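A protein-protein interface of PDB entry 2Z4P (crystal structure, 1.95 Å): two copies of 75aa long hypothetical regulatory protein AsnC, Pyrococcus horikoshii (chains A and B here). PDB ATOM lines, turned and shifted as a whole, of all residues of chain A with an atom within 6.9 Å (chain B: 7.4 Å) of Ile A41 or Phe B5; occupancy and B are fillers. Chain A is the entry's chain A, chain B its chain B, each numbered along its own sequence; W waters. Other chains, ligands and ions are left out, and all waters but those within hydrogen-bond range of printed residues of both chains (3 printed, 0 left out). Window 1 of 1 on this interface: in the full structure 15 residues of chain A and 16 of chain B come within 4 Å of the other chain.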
ATOM      1  N   PHE A   5      -8.699 -20.743 -11.954  1.00  0.00           N
ATOM      2  CA  PHE A   5      -9.431 -20.267 -10.794  1.00  0.00           C
ATOM      3  C   PHE A   5      -8.481 -20.383  -9.615  1.00  0.00           C
ATOM      4  O   PHE A   5      -7.846 -21.421  -9.429  1.00  0.00           O
ATOM      5  CB  PHE A   5     -10.662 -21.130 -10.522  1.00  0.00           C
ATOM      6  CG  PHE A   5     -11.785 -20.898 -11.490  1.00  0.00           C
ATOM      7  CD1 PHE A   5     -11.830 -21.580 -12.700  1.00  0.00           C
ATOM      8  CD2 PHE A   5     -12.783 -19.975 -11.197  1.00  0.00           C
ATOM      9  CE1 PHE A   5     -12.859 -21.343 -13.613  1.00  0.00           C
ATOM     10  CE2 PHE A   5     -13.823 -19.729 -12.101  1.00  0.00           C
ATOM     11  CZ  PHE A   5     -13.858 -20.413 -13.312  1.00  0.00           C
ATOM     12  N   ILE A   6      -8.379 -19.311  -8.837  1.00  0.00           N
ATOM     13  CA  ILE A   6      -7.520 -19.306  -7.668  1.00  0.00           C
ATOM     14  C   ILE A   6      -8.409 -19.152  -6.433  1.00  0.00           C
ATOM     15  O   ILE A   6      -9.169 -18.177  -6.314  1.00  0.00           O
ATOM     16  CB  ILE A   6      -6.525 -18.137  -7.700  1.00  0.00           C
ATOM     17  CG1 ILE A   6      -5.746 -18.138  -9.021  1.00  0.00           C
ATOM     18  CG2 ILE A   6      -5.555 -18.270  -6.516  1.00  0.00           C
ATOM     19  CD1 ILE A   6      -4.831 -16.921  -9.180  1.00  0.00           C
ATOM     20  N   LEU A   7      -8.326 -20.130  -5.537  1.00  0.00           N
ATOM     21  CA  LEU A   7      -9.094 -20.127  -4.295  1.00  0.00           C
ATOM     22  C   LEU A   7      -8.133 -19.571  -3.255  1.00  0.00           C
ATOM     23  O   LEU A   7      -6.973 -19.993  -3.193  1.00  0.00           O
ATOM     24  CB  LEU A   7      -9.488 -21.548  -3.904  1.00  0.00           C
ATOM     25  CG  LEU A   7     -10.148 -22.434  -4.946  1.00  0.00           C
ATOM     26  CD1 LEU A   7     -10.585 -23.737  -4.275  1.00  0.00           C
ATOM     27  CD2 LEU A   7     -11.332 -21.728  -5.558  1.00  0.00           C
ATOM     28  N   MET A   8      -8.607 -18.644  -2.429  1.00  0.00           N
ATOM     29  CA  MET A   8      -7.730 -18.017  -1.456  1.00  0.00           C
ATOM     30  C   MET A   8      -8.314 -17.850  -0.058  1.00  0.00           C
ATOM     31  O   MET A   8      -9.520 -17.649   0.112  1.00  0.00           O
ATOM     32  CB  MET A   8      -7.348 -16.609  -1.926  1.00  0.00           C
ATOM     33  CG  MET A   8      -7.120 -16.439  -3.425  1.00  0.00           C
ATOM     34  SD  MET A   8      -6.782 -14.703  -3.800  1.00  0.00           S
ATOM     35  CE  MET A   8      -6.473 -14.806  -5.601  1.00  0.00           C
ATOM     36  N   MET A  19     -10.448  -8.456  -2.485  1.00  0.00           N
ATOM     37  CA  MET A  19     -11.240  -8.669  -3.698  1.00  0.00           C
ATOM     38  C   MET A  19     -11.262  -7.429  -4.589  1.00  0.00           C
ATOM     39  O   MET A  19     -11.138  -7.526  -5.816  1.00  0.00           O
ATOM     40  CB  MET A  19     -12.686  -9.048  -3.351  1.00  0.00           C
ATOM     41  CG  MET A  19     -13.530  -9.362  -4.583  1.00  0.00           C
ATOM     42  SD  MET A  19     -15.251  -9.705  -4.218  1.00  0.00           S
ATOM     43  CE  MET A  19     -15.815  -8.055  -3.829  1.00  0.00           C
ATOM     44  N   LEU A  22      -7.988  -7.076  -6.416  1.00  0.00           N
ATOM     45  CA  LEU A  22      -7.841  -8.069  -7.471  1.00  0.00           C
ATOM     46  C   LEU A  22      -8.701  -7.726  -8.685  1.00  0.00           C
ATOM     47  O   LEU A  22      -8.241  -7.834  -9.825  1.00  0.00           O
ATOM     48  CB  LEU A  22      -8.213  -9.460  -6.955  1.00  0.00           C
ATOM     49  CG  LEU A  22      -7.296  -9.979  -5.840  1.00  0.00           C
ATOM     50  CD1 LEU A  22      -7.860 -11.271  -5.315  1.00  0.00           C
ATOM     51  CD2 LEU A  22      -5.873 -10.182  -6.364  1.00  0.00           C
ATOM     52  N   GLU A  30     -13.324 -12.364 -12.753  1.00  0.00           N
ATOM     53  CA  GLU A  30     -14.405 -12.463 -11.764  1.00  0.00           C
ATOM     54  C   GLU A  30     -13.794 -12.731 -10.394  1.00  0.00           C
ATOM     55  O   GLU A  30     -12.731 -13.340 -10.296  1.00  0.00           O
ATOM     56  CB  GLU A  30     -15.352 -13.635 -12.055  1.00  0.00           C
ATOM     57  CG  GLU A  30     -15.797 -13.800 -13.477  1.00  0.00           C
ATOM     58  CD  GLU A  30     -16.740 -14.981 -13.641  1.00  0.00           C
ATOM     59  OE1 GLU A  30     -16.870 -15.465 -14.783  1.00  0.00           O
ATOM     60  OE2 GLU A  30     -17.350 -15.414 -12.633  1.00  0.00           O
ATOM     61  N   ALA A  31     -14.477 -12.292  -9.344  1.00  0.00           N
ATOM     62  CA  ALA A  31     -14.003 -12.527  -7.981  1.00  0.00           C
ATOM     63  C   ALA A  31     -15.194 -12.457  -7.049  1.00  0.00           C
ATOM     64  O   ALA A  31     -16.068 -11.601  -7.208  1.00  0.00           O
ATOM     65  CB  ALA A  31     -12.951 -11.510  -7.599  1.00  0.00           C
ATOM     66  N   TYR A  32     -15.243 -13.396  -6.104  1.00  0.00           N
ATOM     67  CA  TYR A  32     -16.336 -13.499  -5.151  1.00  0.00           C
ATOM     68  C   TYR A  32     -15.837 -13.919  -3.781  1.00  0.00           C
ATOM     69  O   TYR A  32     -14.921 -14.749  -3.668  1.00  0.00           O
ATOM     70  CB  TYR A  32     -17.331 -14.583  -5.584  1.00  0.00           C
ATOM     71  CG  TYR A  32     -18.153 -14.265  -6.806  1.00  0.00           C
ATOM     72  CD1 TYR A  32     -19.410 -13.671  -6.685  1.00  0.00           C
ATOM     73  CD2 TYR A  32     -17.701 -14.617  -8.076  1.00  0.00           C
ATOM     74  CE1 TYR A  32     -20.210 -13.449  -7.804  1.00  0.00           C
ATOM     75  CE2 TYR A  32     -18.492 -14.397  -9.207  1.00  0.00           C
ATOM     76  CZ  TYR A  32     -19.744 -13.820  -9.061  1.00  0.00           C
ATOM     77  OH  TYR A  32     -20.553 -13.658 -10.163  1.00  0.00           O
ATOM     78  N   VAL A  33     -16.442 -13.343  -2.749  1.00  0.00           N
ATOM     79  CA  VAL A  33     -16.133 -13.727  -1.374  1.00  0.00           C
ATOM     80  C   VAL A  33     -17.057 -14.917  -1.172  1.00  0.00           C
ATOM     81  O   VAL A  33     -18.228 -14.871  -1.575  1.00  0.00           O
ATOM     82  CB  VAL A  33     -16.510 -12.613  -0.390  1.00  0.00           C
ATOM     83  CG1 VAL A  33     -16.438 -13.138   1.050  1.00  0.00           C
ATOM     84  CG2 VAL A  33     -15.564 -11.439  -0.581  1.00  0.00           C
ATOM     85  N   VAL A  34     -16.561 -15.983  -0.551  1.00  0.00           N
ATOM     86  CA  VAL A  34     -17.378 -17.172  -0.383  1.00  0.00           C
ATOM     87  C   VAL A  34     -17.303 -17.795   1.007  1.00  0.00           C
ATOM     88  O   VAL A  34     -16.371 -17.542   1.753  1.00  0.00           O
ATOM     89  CB  VAL A  34     -16.959 -18.263  -1.403  1.00  0.00           C
ATOM     90  CG1 VAL A  34     -17.324 -17.822  -2.839  1.00  0.00           C
ATOM     91  CG2 VAL A  34     -15.447 -18.491  -1.317  1.00  0.00           C
ATOM     92  N   TYR A  38     -12.251 -21.697   2.009  1.00  0.00           N
ATOM     93  CA  TYR A  38     -11.645 -20.626   1.230  1.00  0.00           C
ATOM     94  C   TYR A  38     -12.492 -19.370   1.422  1.00  0.00           C
ATOM     95  O   TYR A  38     -13.683 -19.472   1.701  1.00  0.00           O
ATOM     96  CB  TYR A  38     -11.586 -21.028  -0.241  1.00  0.00           C
ATOM     97  CG  TYR A  38     -10.573 -22.117  -0.475  1.00  0.00           C
ATOM     98  CD1 TYR A  38      -9.207 -21.839  -0.400  1.00  0.00           C
ATOM     99  CD2 TYR A  38     -10.971 -23.428  -0.709  1.00  0.00           C
ATOM    100  CE1 TYR A  38      -8.259 -22.841  -0.548  1.00  0.00           C
ATOM    101  CE2 TYR A  38     -10.025 -24.449  -0.860  1.00  0.00           C
ATOM    102  CZ  TYR A  38      -8.672 -24.142  -0.776  1.00  0.00           C
ATOM    103  OH  TYR A  38      -7.721 -25.128  -0.918  1.00  0.00           O
ATOM    104  N   ASP A  39     -11.876 -18.200   1.274  1.00  0.00           N
ATOM    105  CA  ASP A  39     -12.580 -16.933   1.469  1.00  0.00           C
ATOM    106  C   ASP A  39     -12.912 -16.211   0.179  1.00  0.00           C
ATOM    107  O   ASP A  39     -13.885 -15.450   0.127  1.00  0.00           O
ATOM    108  CB  ASP A  39     -11.750 -16.006   2.351  1.00  0.00           C
ATOM    109  CG  ASP A  39     -11.428 -16.630   3.688  1.00  0.00           C
ATOM    110  OD1 ASP A  39     -12.260 -17.430   4.149  1.00  0.00           O
ATOM    111  OD2 ASP A  39     -10.366 -16.324   4.265  1.00  0.00           O
ATOM    112  N   LEU A  40     -12.077 -16.421  -0.842  1.00  0.00           N
ATOM    113  CA  LEU A  40     -12.286 -15.793  -2.155  1.00  0.00           C
ATOM    114  C   LEU A  40     -12.043 -16.804  -3.257  1.00  0.00           C
ATOM    115  O   LEU A  40     -11.224 -17.726  -3.106  1.00  0.00           O
ATOM    116  CB  LEU A  40     -11.289 -14.642  -2.403  1.00  0.00           C
ATOM    117  CG  LEU A  40     -11.241 -13.364  -1.563  1.00  0.00           C
ATOM    118  CD1 LEU A  40     -10.108 -12.464  -2.043  1.00  0.00           C
ATOM    119  CD2 LEU A  40     -12.559 -12.636  -1.679  1.00  0.00           C
ATOM    120  N   ILE A  41     -12.767 -16.640  -4.362  1.00  0.00           N
ATOM    121  CA  ILE A  41     -12.536 -17.461  -5.536  1.00  0.00           C
ATOM    122  C   ILE A  41     -12.322 -16.404  -6.613  1.00  0.00           C
ATOM    123  O   ILE A  41     -13.089 -15.435  -6.730  1.00  0.00           O
ATOM    124  CB  ILE A  41     -13.708 -18.393  -5.930  1.00  0.00           C
ATOM    125  CG1 ILE A  41     -13.360 -19.075  -7.265  1.00  0.00           C
ATOM    126  CG2 ILE A  41     -14.992 -17.615  -6.089  1.00  0.00           C
ATOM    127  CD1 ILE A  41     -13.996 -20.440  -7.460  1.00  0.00           C
ATOM    128  N   VAL A  42     -11.257 -16.574  -7.381  1.00  0.00           N
ATOM    129  CA  VAL A  42     -10.923 -15.608  -8.399  1.00  0.00           C
ATOM    130  C   VAL A  42     -10.689 -16.305  -9.725  1.00  0.00           C
ATOM    131  O   VAL A  42     -10.008 -17.323  -9.781  1.00  0.00           O
ATOM    132  CB  VAL A  42      -9.648 -14.851  -7.975  1.00  0.00           C
ATOM    133  CG1 VAL A  42      -9.326 -13.763  -8.961  1.00  0.00           C
ATOM    134  CG2 VAL A  42      -9.840 -14.281  -6.573  1.00  0.00           C
ATOM    135  N   LYS A  43     -11.274 -15.768 -10.788  1.00  0.00           N
ATOM    136  CA  LYS A  43     -11.077 -16.344 -12.105  1.00  0.00           C
ATOM    137  C   LYS A  43     -10.098 -15.451 -12.846  1.00  0.00           C
ATOM    138  O   LYS A  43     -10.293 -14.234 -12.921  1.00  0.00           O
ATOM    139  CB  LYS A  43     -12.386 -16.382 -12.876  1.00  0.00           C
ATOM    140  CG  LYS A  43     -12.283 -17.041 -14.229  1.00  0.00           C
ATOM    141  CD  LYS A  43     -13.662 -16.984 -14.891  1.00  0.00           C
ATOM    142  CE  LYS A  43     -13.583 -17.313 -16.352  1.00  0.00           C
ATOM    143  NZ  LYS A  43     -14.931 -17.303 -16.991  1.00  0.00           N
ATOM    144  N   MET A  72      -6.352 -23.852  -9.789  1.00  0.00           N
ATOM    145  CA  MET A  72      -6.819 -24.909 -10.675  1.00  0.00           C
ATOM    146  C   MET A  72      -6.872 -24.321 -12.084  1.00  0.00           C
ATOM    147  O   MET A  72      -7.588 -23.350 -12.339  1.00  0.00           O
ATOM    148  CB  MET A  72      -8.200 -25.396 -10.230  1.00  0.00           C
ATOM    149  CG  MET A  72      -8.168 -26.062  -8.852  1.00  0.00           C
ATOM    150  SD  MET A  72      -9.802 -26.323  -8.187  1.00  0.00           S
ATOM    151  CE  MET A  72     -10.138 -24.718  -7.542  1.00  0.00           C
ATOM    152  N   THR B   3     -25.519 -17.153  -5.718  1.00  0.00           N
ATOM    153  CA  THR B   3     -24.467 -17.636  -6.608  1.00  0.00           C
ATOM    154  C   THR B   3     -23.580 -18.565  -5.794  1.00  0.00           C
ATOM    155  O   THR B   3     -23.296 -18.286  -4.618  1.00  0.00           O
ATOM    156  CB  THR B   3     -23.600 -16.474  -7.144  1.00  0.00           C
ATOM    157  OG1 THR B   3     -24.425 -15.546  -7.858  1.00  0.00           O
ATOM    158  CG2 THR B   3     -22.513 -17.007  -8.082  1.00  0.00           C
ATOM    159  N   ALA B   4     -23.147 -19.667  -6.407  1.00  0.00           N
ATOM    160  CA  ALA B   4     -22.278 -20.611  -5.721  1.00  0.00           C
ATOM    161  C   ALA B   4     -21.322 -21.268  -6.715  1.00  0.00           C
ATOM    162  O   ALA B   4     -21.594 -21.334  -7.923  1.00  0.00           O
ATOM    163  CB  ALA B   4     -23.123 -21.685  -5.009  1.00  0.00           C
ATOM    164  N   PHE B   5     -20.191 -21.728  -6.206  1.00  0.00           N
ATOM    165  CA  PHE B   5     -19.229 -22.433  -7.038  1.00  0.00           C
ATOM    166  C   PHE B   5     -19.125 -23.848  -6.490  1.00  0.00           C
ATOM    167  O   PHE B   5     -18.857 -24.043  -5.296  1.00  0.00           O
ATOM    168  CB  PHE B   5     -17.860 -21.734  -6.997  1.00  0.00           C
ATOM    169  CG  PHE B   5     -17.816 -20.454  -7.775  1.00  0.00           C
ATOM    170  CD1 PHE B   5     -18.253 -19.261  -7.209  1.00  0.00           C
ATOM    171  CD2 PHE B   5     -17.358 -20.446  -9.089  1.00  0.00           C
ATOM    172  CE1 PHE B   5     -18.231 -18.080  -7.940  1.00  0.00           C
ATOM    173  CE2 PHE B   5     -17.333 -19.267  -9.837  1.00  0.00           C
ATOM    174  CZ  PHE B   5     -17.771 -18.079  -9.258  1.00  0.00           C
ATOM    175  N   ILE B   6     -19.357 -24.837  -7.354  1.00  0.00           N
ATOM    176  CA  ILE B   6     -19.276 -26.226  -6.946  1.00  0.00           C
ATOM    177  C   ILE B   6     -17.959 -26.808  -7.431  1.00  0.00           C
ATOM    178  O   ILE B   6     -17.655 -26.755  -8.633  1.00  0.00           O
ATOM    179  CB  ILE B   6     -20.378 -27.110  -7.574  1.00  0.00           C
ATOM    180  CG1 ILE B   6     -21.760 -26.503  -7.358  1.00  0.00           C
ATOM    181  CG2 ILE B   6     -20.310 -28.502  -6.964  1.00  0.00           C
ATOM    182  CD1 ILE B   6     -22.843 -27.209  -8.150  1.00  0.00           C
ATOM    183  N   LEU B   7     -17.184 -27.354  -6.498  1.00  0.00           N
ATOM    184  CA  LEU B   7     -15.918 -28.007  -6.827  1.00  0.00           C
ATOM    185  C   LEU B   7     -16.305 -29.486  -6.844  1.00  0.00           C
ATOM    186  O   LEU B   7     -16.862 -29.997  -5.864  1.00  0.00           O
ATOM    187  CB  LEU B   7     -14.879 -27.740  -5.738  1.00  0.00           C
ATOM    188  CG  LEU B   7     -14.587 -26.266  -5.434  1.00  0.00           C
ATOM    189  CD1 LEU B   7     -13.572 -26.162  -4.299  1.00  0.00           C
ATOM    190  CD2 LEU B   7     -14.071 -25.564  -6.700  1.00  0.00           C
ATOM    191  N   MET B   8     -16.017 -30.177  -7.943  1.00  0.00           N
ATOM    192  CA  MET B   8     -16.412 -31.576  -8.059  1.00  0.00           C
ATOM    193  C   MET B   8     -15.317 -32.575  -8.375  1.00  0.00           C
ATOM    194  O   MET B   8     -14.309 -32.237  -8.990  1.00  0.00           O
ATOM    195  CB  MET B   8     -17.445 -31.757  -9.174  1.00  0.00           C
ATOM    196  CG  MET B   8     -18.735 -31.018  -9.046  1.00  0.00           C
ATOM    197  SD  MET B   8     -19.725 -31.414 -10.524  1.00  0.00           S
ATOM    198  CE  MET B   8     -21.100 -30.342 -10.254  1.00  0.00           C
ATOM    199  N   GLU B  30     -21.428 -21.413 -15.641  1.00  0.00           N
ATOM    200  CA  GLU B  30     -20.081 -21.674 -16.152  1.00  0.00           C
ATOM    201  C   GLU B  30     -19.645 -23.042 -15.646  1.00  0.00           C
ATOM    202  O   GLU B  30     -19.971 -23.417 -14.519  1.00  0.00           O
ATOM    203  CB  GLU B  30     -19.058 -20.639 -15.641  1.00  0.00           C
ATOM    204  CG  GLU B  30     -19.408 -19.170 -15.870  1.00  0.00           C
ATOM    205  CD  GLU B  30     -18.312 -18.215 -15.404  1.00  0.00           C
ATOM    206  OE1 GLU B  30     -18.633 -17.035 -15.150  1.00  0.00           O
ATOM    207  OE2 GLU B  30     -17.131 -18.628 -15.306  1.00  0.00           O
ATOM    208  N   LEU B  40     -13.820 -30.698 -11.730  1.00  0.00           N
ATOM    209  CA  LEU B  40     -14.584 -29.623 -12.351  1.00  0.00           C
ATOM    210  C   LEU B  40     -14.888 -28.498 -11.379  1.00  0.00           C
ATOM    211  O   LEU B  40     -14.971 -28.709 -10.166  1.00  0.00           O
ATOM    212  CB  LEU B  40     -15.925 -30.143 -12.876  1.00  0.00           C
ATOM    213  CG  LEU B  40     -16.005 -31.242 -13.932  1.00  0.00           C
ATOM    214  CD1 LEU B  40     -17.469 -31.596 -14.165  1.00  0.00           C
ATOM    215  CD2 LEU B  40     -15.375 -30.763 -15.223  1.00  0.00           C
ATOM    216  N   ILE B  41     -15.029 -27.298 -11.926  1.00  0.00           N
ATOM    217  CA  ILE B  41     -15.431 -26.130 -11.154  1.00  0.00           C
ATOM    218  C   ILE B  41     -16.654 -25.640 -11.917  1.00  0.00           C
ATOM    219  O   ILE B  41     -16.592 -25.404 -13.135  1.00  0.00           O
ATOM    220  CB  ILE B  41     -14.361 -25.041 -11.120  1.00  0.00           C
ATOM    221  CG1 ILE B  41     -13.130 -25.571 -10.382  1.00  0.00           C
ATOM    222  CG2 ILE B  41     -14.890 -23.814 -10.354  1.00  0.00           C
ATOM    223  CD1 ILE B  41     -12.016 -24.547 -10.217  1.00  0.00           C
ATOM    224  N   VAL B  42     -17.764 -25.501 -11.204  1.00  0.00           N
ATOM    225  CA  VAL B  42     -19.029 -25.111 -11.813  1.00  0.00           C
ATOM    226  C   VAL B  42     -19.663 -23.921 -11.107  1.00  0.00           C
ATOM    227  O   VAL B  42     -19.821 -23.933  -9.878  1.00  0.00           O
ATOM    228  CB  VAL B  42     -20.015 -26.291 -11.735  1.00  0.00           C
ATOM    229  CG1 VAL B  42     -21.262 -26.007 -12.569  1.00  0.00           C
ATOM    230  CG2 VAL B  42     -19.318 -27.586 -12.189  1.00  0.00           C
ATOM    231  N   LYS B  43     -20.026 -22.895 -11.877  1.00  0.00           N
ATOM    232  CA  LYS B  43     -20.673 -21.722 -11.295  1.00  0.00           C
ATOM    233  C   LYS B  43     -22.175 -21.890 -11.492  1.00  0.00           C
ATOM    234  O   LYS B  43     -22.637 -22.121 -12.608  1.00  0.00           O
ATOM    235  CB  LYS B  43     -20.203 -20.435 -11.989  1.00  0.00           C
ATOM    236  CG  LYS B  43     -20.826 -19.143 -11.409  1.00  0.00           C
ATOM    237  CD  LYS B  43     -20.406 -17.917 -12.234  1.00  0.00           C
ATOM    238  CE  LYS B  43     -20.940 -16.618 -11.623  1.00  0.00           C
ATOM    239  NZ  LYS B  43     -20.412 -15.412 -12.330  1.00  0.00           N
ATOM    240  N   VAL B  44     -22.936 -21.788 -10.411  1.00  0.00           N
ATOM    241  CA  VAL B  44     -24.373 -21.929 -10.520  1.00  0.00           C
ATOM    242  C   VAL B  44     -25.070 -20.739  -9.876  1.00  0.00           C
ATOM    243  O   VAL B  44     -24.509 -20.074  -8.999  1.00  0.00           O
ATOM    244  CB  VAL B  44     -24.857 -23.246  -9.858  1.00  0.00           C
ATOM    245  CG1 VAL B  44     -24.124 -24.428 -10.474  1.00  0.00           C
ATOM    246  CG2 VAL B  44     -24.609 -23.213  -8.343  1.00  0.00           C
ATOM    247  N   LEU B  52     -31.314 -23.632  -4.311  1.00  0.00           N
ATOM    248  CA  LEU B  52     -29.960 -24.169  -4.428  1.00  0.00           C
ATOM    249  C   LEU B  52     -29.896 -25.469  -3.617  1.00  0.00           C
ATOM    250  O   LEU B  52     -29.358 -26.470  -4.081  1.00  0.00           O
ATOM    251  CB  LEU B  52     -28.933 -23.177  -3.876  1.00  0.00           C
ATOM    252  CG  LEU B  52     -27.496 -23.705  -3.932  1.00  0.00           C
ATOM    253  CD1 LEU B  52     -27.065 -23.756  -5.407  1.00  0.00           C
ATOM    254  CD2 LEU B  52     -26.553 -22.787  -3.129  1.00  0.00           C
ATOM    255  N   ILE B  56     -28.674 -28.877  -5.479  1.00  0.00           N
ATOM    256  CA  ILE B  56     -27.480 -29.627  -5.123  1.00  0.00           C
ATOM    257  C   ILE B  56     -27.775 -31.025  -4.588  1.00  0.00           C
ATOM    258  O   ILE B  56     -27.151 -31.995  -5.017  1.00  0.00           O
ATOM    259  CB  ILE B  56     -26.617 -28.875  -4.084  1.00  0.00           C
ATOM    260  CG1 ILE B  56     -26.235 -27.493  -4.614  1.00  0.00           C
ATOM    261  CG2 ILE B  56     -25.351 -29.677  -3.786  1.00  0.00           C
ATOM    262  CD1 ILE B  56     -25.396 -27.531  -5.868  1.00  0.00           C
ATOM    263  N   SER B  70     -18.124 -30.001  -3.226  1.00  0.00           N
ATOM    264  CA  SER B  70     -17.859 -29.063  -2.145  1.00  0.00           C
ATOM    265  C   SER B  70     -18.365 -27.746  -2.734  1.00  0.00           C
ATOM    266  O   SER B  70     -17.754 -27.186  -3.649  1.00  0.00           O
ATOM    267  CB  SER B  70     -16.362 -29.003  -1.840  1.00  0.00           C
ATOM    268  OG  SER B  70     -16.105 -28.062  -0.816  1.00  0.00           O
ATOM    269  N   THR B  71     -19.501 -27.272  -2.228  1.00  0.00           N
ATOM    270  CA  THR B  71     -20.125 -26.060  -2.746  1.00  0.00           C
ATOM    271  C   THR B  71     -19.819 -24.818  -1.905  1.00  0.00           C
ATOM    272  O   THR B  71     -19.999 -24.810  -0.679  1.00  0.00           O
ATOM    273  CB  THR B  71     -21.655 -26.282  -2.869  1.00  0.00           C
ATOM    274  OG1 THR B  71     -21.893 -27.429  -3.699  1.00  0.00           O
ATOM    275  CG2 THR B  71     -22.342 -25.071  -3.494  1.00  0.00           C
ATOM    276  N   MET B  72     -19.337 -23.776  -2.578  1.00  0.00           N
ATOM    277  CA  MET B  72     -18.979 -22.519  -1.933  1.00  0.00           C
ATOM    278  C   MET B  72     -19.970 -21.431  -2.316  1.00  0.00           C
ATOM    279  O   MET B  72     -19.946 -20.911  -3.438  1.00  0.00           O
ATOM    280  CB  MET B  72     -17.568 -22.100  -2.360  1.00  0.00           C
ATOM    281  CG  MET B  72     -16.515 -23.167  -2.015  1.00  0.00           C
ATOM    282  SD  MET B  72     -14.873 -22.733  -2.590  1.00  0.00           S
ATOM    283  CE  MET B  72     -15.050 -23.079  -4.335  1.00  0.00           C
ATOM    284  N   ILE B  73     -20.845 -21.090  -1.380  1.00  0.00           N
ATOM    285  CA  ILE B  73     -21.854 -20.054  -1.617  1.00  0.00           C
ATOM    286  C   ILE B  73     -21.210 -18.674  -1.556  1.00  0.00           C
ATOM    287  O   ILE B  73     -20.429 -18.387  -0.650  1.00  0.00           O
ATOM    288  CB  ILE B  73     -22.972 -20.167  -0.557  1.00  0.00           C
ATOM    289  CG1 ILE B  73     -23.698 -21.499  -0.746  1.00  0.00           C
ATOM    290  CG2 ILE B  73     -23.922 -18.969  -0.649  1.00  0.00           C
ATOM    291  CD1 ILE B  73     -24.713 -21.832   0.335  1.00  0.00           C
ATOM    292  N   ALA B  74     -21.527 -17.810  -2.521  1.00  0.00           N
ATOM    293  CA  ALA B  74     -20.948 -16.478  -2.544  1.00  0.00           C
ATOM    294  C   ALA B  74     -21.733 -15.484  -1.716  1.00  0.00           C
ATOM    295  O   ALA B  74     -22.959 -15.602  -1.569  1.00  0.00           O
ATOM    296  CB  ALA B  74     -20.845 -15.956  -3.982  1.00  0.00           C
HETATM  297  O   HOH W   1     -23.184 -13.638  -9.599  1.00  0.00           O
HETATM  298  O   HOH W   2     -21.627 -12.433 -12.701  1.00  0.00           O
HETATM  299  O   HOH W   3     -14.987 -21.555   0.758  1.00  0.00           O
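NZ of Lys B43 is in salt-bridge range of OE2 of Glu A30, at 3.1 Å.
The side-chain amino group of Lys A43 lies within salt-bridge range of the side-chain carboxylate of Glu B30 (3.1 Å).
OH of Tyr A32 is in hydrogen-bond range of NZ of Lys B43, 2.8 Å away.
The side-chain carboxylate of Glu B30 sits close to the side-chain carboxylate of Glu A30 (2.4 Å).
The backbone carbonyl oxygen (O) of Met A72 lies within hydrogen-bond range of the backbone NH (N) of Phe A5, 2.9 Å away.
O of Ser B70 lies within hydrogen-bond range of N of Leu B7 (2.9 Å).
The backbone carbonyl oxygen of Thr B3 sits at hydrogen-bond distance from the backbone NH of Ala B74, at 2.8 Å.
The backbone carbonyl oxygen of Phe B5 sits at hydrogen-bond distance from the backbone NH of Met B72.
The backbone NH (N) of Ile A41 sits at hydrogen-bond distance from the backbone carbonyl oxygen (O) of Tyr A32.
The side-chain carboxylate of Glu B30 lies within salt-bridge range of the side-chain amino group of Lys B43.
Phe A5 touches Ile B41.
CD1 of Leu A7 touches CD1 of Leu B7, 3.8 Å away.
Tyr A32 touches Phe B5 (CD2 to CE1, 3.5 Å).
Ala B74 touches Tyr A32 (CB to CD1, 3.8 Å).
Val A33 touches Ala B74 (O to CA, 3.3 Å).
Ile B73 touches Val A34.
Ala B74 touches Val A34.
Ile A41 touches Phe B5.
CE of Met A72 touches CD1 of Ile B41, 3.3 Å away.
Of the printed residues of chain B, Ile A41 touches Phe B5.
Of the printed residues of chain A, Phe B5 touches Tyr A32 and Ile A41.
Printed residues of chain A within 4 Å of Leu B7: Leu A7 (3.8 Å).
Of the printed residues of chain B, Leu A7 touches Leu B7.
Printed residues of chain B within 4 Å of Met A72: Ile B41.
Of the printed residues of chain B, Phe A5 touches Ile B41 (3.7 Å).
Ile A6 touches none of the printed residues of chain B.
Met B72 touches none of the printed residues of chain A.
The nearest residue of chain B that does not touch Ile A41 is Met B72 (4.2 Å).
The nearest residue of chain A that does not touch Phe B5 is Phe A5 (4.2 Å).
The nearest printed residue of chain A that does not touch Ile B73 is Val A33 (4.2 Å).
Of the 19 printed residues of chain B, 7 touch a printed residue of chain A.
Hydrophobic or aromatic side chains of chain B within 4 Å of the printed part of chain A: Phe B5, Leu B7, Ile B41 and Ala B74.
Along chain B the printed residues that touch a printed residue of chain A span positions 5 to 74.
Hydrophobic or aromatic side chains of chain A within 4 Å of the printed part of chain B: Phe A5, Leu A7, Tyr A32, Val A34, Ile A41 and Met A72.
Among the printed residues, 13 pairs touch across the chains.
Among the printed residues, Asp or Glu carboxylates within 4 Å of a Lys or Arg side-chain nitrogen of the other chain: Glu A30 with Lys B43 and Lys A43 with Glu B30.
Phe A5 touches Ile B41, and with the chains exchanged Ile A41 touches Phe B5.
Leu A7 touches its own counterpart, Leu B7.
Glu B30 touches its own counterpart, Glu A30.
Met A72 touches Ile B41, but with the chains exchanged Ile A41 does not touch Met B72 (4.2 Å).
Positions printed for both chains: 5, 6, 7, 8, 30, 40, 41, 42, 43 and 72.
Of the 13 pairs that touch across the chains among the printed residues, 6 have their exchanged pair printed and touching as well.
Water W3 bridges O of Tyr A38 (2.6 Å) and SD of Met B72 (3.6 Å).
Water W1 bridges the side-chain hydroxyl of Tyr A32 and the side-chain hydroxyl of Thr B3.
Water W2 lies within hydrogen-bond range of the side-chain hydroxyl (OH) of Tyr A32 (3.0 Å) and the side-chain amino group (NZ) of Lys B43 (3.2 Å).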
